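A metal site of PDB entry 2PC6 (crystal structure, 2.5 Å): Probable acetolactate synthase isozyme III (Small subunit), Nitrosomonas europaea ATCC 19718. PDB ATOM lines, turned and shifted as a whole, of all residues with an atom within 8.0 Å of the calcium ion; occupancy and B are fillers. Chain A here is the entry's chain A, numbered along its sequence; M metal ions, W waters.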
ATOM      1  N   LEU A  10     -15.450  35.014 -10.863  1.00  0.00           N
ATOM      2  CA  LEU A  10     -14.714  35.213  -9.657  1.00  0.00           C
ATOM      3  C   LEU A  10     -13.328  34.601  -9.817  1.00  0.00           C
ATOM      4  O   LEU A  10     -13.159  33.456 -10.247  1.00  0.00           O
ATOM      5  CB  LEU A  10     -15.452  34.564  -8.481  1.00  0.00           C
ATOM      6  CG  LEU A  10     -16.546  35.316  -7.701  1.00  0.00           C
ATOM      7  CD1 LEU A  10     -17.008  34.470  -6.546  1.00  0.00           C
ATOM      8  CD2 LEU A  10     -16.166  36.729  -7.199  1.00  0.00           C
ATOM      9  N   LYS A  64     -16.040  26.488 -21.081  1.00  0.00           N
ATOM     10  CA  LYS A  64     -15.497  25.230 -20.654  1.00  0.00           C
ATOM     11  C   LYS A  64     -14.016  25.450 -20.268  1.00  0.00           C
ATOM     12  O   LYS A  64     -13.629  25.169 -19.129  1.00  0.00           O
ATOM     13  CB  LYS A  64     -15.704  24.122 -21.701  1.00  0.00           C
ATOM     14  N   GLN A  65     -13.221  25.998 -21.191  1.00  0.00           N
ATOM     15  CA  GLN A  65     -11.803  26.201 -20.879  1.00  0.00           C
ATOM     16  C   GLN A  65     -11.571  27.102 -19.674  1.00  0.00           C
ATOM     17  O   GLN A  65     -10.645  26.858 -18.897  1.00  0.00           O
ATOM     18  CB  GLN A  65     -11.016  26.757 -22.058  1.00  0.00           C
ATOM     19  CG  GLN A  65     -10.664  25.804 -23.169  1.00  0.00           C
ATOM     20  CD  GLN A  65     -10.147  26.590 -24.389  1.00  0.00           C
ATOM     21  OE1 GLN A  65     -10.832  26.726 -25.410  1.00  0.00           O
ATOM     22  NE2 GLN A  65      -8.969  27.189 -24.230  1.00  0.00           N
ATOM     23  N   LEU A  66     -12.397  28.132 -19.491  1.00  0.00           N
ATOM     24  CA  LEU A  66     -12.148  29.034 -18.365  1.00  0.00           C
ATOM     25  C   LEU A  66     -12.321  28.352 -17.010  1.00  0.00           C
ATOM     26  O   LEU A  66     -11.530  28.580 -16.082  1.00  0.00           O
ATOM     27  CB  LEU A  66     -13.026  30.290 -18.444  1.00  0.00           C
ATOM     28  CG  LEU A  66     -12.550  31.447 -19.313  1.00  0.00           C
ATOM     29  CD1 LEU A  66     -13.710  32.360 -19.606  1.00  0.00           C
ATOM     30  CD2 LEU A  66     -11.514  32.190 -18.584  1.00  0.00           C
ATOM     31  N   ASN A  67     -13.359  27.528 -16.901  1.00  0.00           N
ATOM     32  CA  ASN A  67     -13.639  26.835 -15.651  1.00  0.00           C
ATOM     33  C   ASN A  67     -12.523  25.898 -15.246  1.00  0.00           C
ATOM     34  O   ASN A  67     -12.305  25.699 -14.058  1.00  0.00           O
ATOM     35  CB  ASN A  67     -14.978  26.090 -15.700  1.00  0.00           C
ATOM     36  CG  ASN A  67     -16.119  26.928 -15.150  1.00  0.00           C
ATOM     37  OD1 ASN A  67     -17.198  27.045 -15.781  1.00  0.00           O
ATOM     38  ND2 ASN A  67     -15.903  27.518 -13.975  1.00  0.00           N
ATOM     39  N   LYS A  68     -11.807  25.362 -16.247  1.00  0.00           N
ATOM     40  CA  LYS A  68     -10.703  24.455 -16.025  1.00  0.00           C
ATOM     41  C   LYS A  68      -9.549  25.143 -15.295  1.00  0.00           C
ATOM     42  O   LYS A  68      -8.839  24.470 -14.539  1.00  0.00           O
ATOM     43  CB  LYS A  68     -10.178  23.861 -17.354  1.00  0.00           C
ATOM     44  CG  LYS A  68     -10.811  22.526 -17.771  1.00  0.00           C
ATOM     45  N   LEU A  69      -9.337  26.445 -15.539  1.00  0.00           N
ATOM     46  CA  LEU A  69      -8.273  27.187 -14.859  1.00  0.00           C
ATOM     47  C   LEU A  69      -8.530  27.120 -13.378  1.00  0.00           C
ATOM     48  O   LEU A  69      -9.647  27.319 -12.953  1.00  0.00           O
ATOM     49  CB  LEU A  69      -8.262  28.658 -15.300  1.00  0.00           C
ATOM     50  CG  LEU A  69      -8.030  28.991 -16.771  1.00  0.00           C
ATOM     51  CD1 LEU A  69      -8.032  30.493 -17.003  1.00  0.00           C
ATOM     52  CD2 LEU A  69      -6.706  28.379 -17.286  1.00  0.00           C
ATOM     53  N   ILE A  70      -7.508  26.811 -12.571  1.00  0.00           N
ATOM     54  CA  ILE A  70      -7.730  26.772 -11.095  1.00  0.00           C
ATOM     55  C   ILE A  70      -8.007  28.165 -10.458  1.00  0.00           C
ATOM     56  O   ILE A  70      -8.603  28.242  -9.384  1.00  0.00           O
ATOM     57  CB  ILE A  70      -6.630  26.004 -10.278  1.00  0.00           C
ATOM     58  CG1 ILE A  70      -5.284  26.725 -10.321  1.00  0.00           C
ATOM     59  CG2 ILE A  70      -6.539  24.539 -10.708  1.00  0.00           C
ATOM     60  N   GLU A  71      -7.586  29.229 -11.121  1.00  0.00           N
ATOM     61  CA  GLU A  71      -7.751  30.574 -10.557  1.00  0.00           C
ATOM     62  C   GLU A  71      -9.147  31.156 -10.813  1.00  0.00           C
ATOM     63  O   GLU A  71      -9.528  32.173 -10.219  1.00  0.00           O
ATOM     64  CB  GLU A  71      -6.645  31.517 -11.053  1.00  0.00           C
ATOM     65  CG  GLU A  71      -5.272  31.298 -10.396  1.00  0.00           C
ATOM     66  CD  GLU A  71      -4.133  31.950 -11.185  1.00  0.00           C
ATOM     67  OE1 GLU A  71      -4.252  32.124 -12.415  1.00  0.00           O
ATOM     68  OE2 GLU A  71      -3.106  32.267 -10.566  1.00  0.00           O
ATOM     69  N   VAL A  72      -9.903  30.486 -11.691  1.00  0.00           N
ATOM     70  CA  VAL A  72     -11.281  30.814 -11.935  1.00  0.00           C
ATOM     71  C   VAL A  72     -12.171  29.961 -11.020  1.00  0.00           C
ATOM     72  O   VAL A  72     -12.184  28.748 -11.097  1.00  0.00           O
ATOM     73  CB  VAL A  72     -11.581  30.545 -13.385  1.00  0.00           C
ATOM     74  CG1 VAL A  72     -13.118  30.510 -13.639  1.00  0.00           C
ATOM     75  CG2 VAL A  72     -10.850  31.602 -14.281  1.00  0.00           C
ATOM     76  N   VAL A  73     -12.922  30.622 -10.156  1.00  0.00           N
ATOM     77  CA  VAL A  73     -13.548  29.954  -9.007  1.00  0.00           C
ATOM     78  C   VAL A  73     -15.043  29.662  -9.245  1.00  0.00           C
ATOM     79  O   VAL A  73     -15.519  28.562  -8.973  1.00  0.00           O
ATOM     80  CB  VAL A  73     -13.351  30.793  -7.682  1.00  0.00           C
ATOM     81  CG1 VAL A  73     -14.135  30.171  -6.531  1.00  0.00           C
ATOM     82  CG2 VAL A  73     -11.858  30.909  -7.317  1.00  0.00           C
ATOM     83  N   LYS A  74     -15.768  30.681  -9.715  1.00  0.00           N
ATOM     84  CA  LYS A  74     -17.142  30.558 -10.175  1.00  0.00           C
ATOM     85  C   LYS A  74     -17.238  31.351 -11.471  1.00  0.00           C
ATOM     86  O   LYS A  74     -16.383  32.204 -11.769  1.00  0.00           O
ATOM     87  CB  LYS A  74     -18.161  31.040  -9.119  1.00  0.00           C
ATOM     88  CG  LYS A  74     -18.667  29.923  -8.155  1.00  0.00           C
ATOM     89  N   LEU A  75     -18.305  31.116 -12.235  1.00  0.00           N
ATOM     90  CA  LEU A  75     -18.423  31.668 -13.575  1.00  0.00           C
ATOM     91  C   LEU A  75     -19.857  31.485 -14.057  1.00  0.00           C
ATOM     92  O   LEU A  75     -20.411  30.390 -13.957  1.00  0.00           O
ATOM     93  CB  LEU A  75     -17.470  30.915 -14.528  1.00  0.00           C
ATOM     94  CG  LEU A  75     -17.425  31.438 -15.971  1.00  0.00           C
ATOM     95  CD1 LEU A  75     -16.111  31.148 -16.664  1.00  0.00           C
ATOM     96  CD2 LEU A  75     -18.626  30.911 -16.790  1.00  0.00           C
HETATM   97 CA    CA M   1     -11.733  26.410 -11.840  1.00  0.00          CA
HETATM   98  O   HOH W   1     -10.906  26.274  -9.518  1.00  0.00           O
HETATM   99  O   HOH W   2     -12.670  24.611 -10.852  1.00  0.00           O
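Water W2 is bound to the calcium ion (2.3 Å).
The calcium ion is bound by O of Asn 67, at 2.4 Å.
Water W1 is bound to the calcium ion, at 2.5 Å.
The backbone carbonyl oxygen (O) of Val 72 binds the calcium ion, at 2.5 Å.
The calcium ion is bound by O of Leu 69 (2.5 Å).
The calcium ion has five donor atoms within binding distance.
Of the 13 residues printed, 3 come within 4 Å of the calcium ion.
Along chain A the residues within 4 Å of the calcium ion span positions 67 to 72.
The nearest printed residue that does not touch the calcium ion is Ile 70 (4.1 Å).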
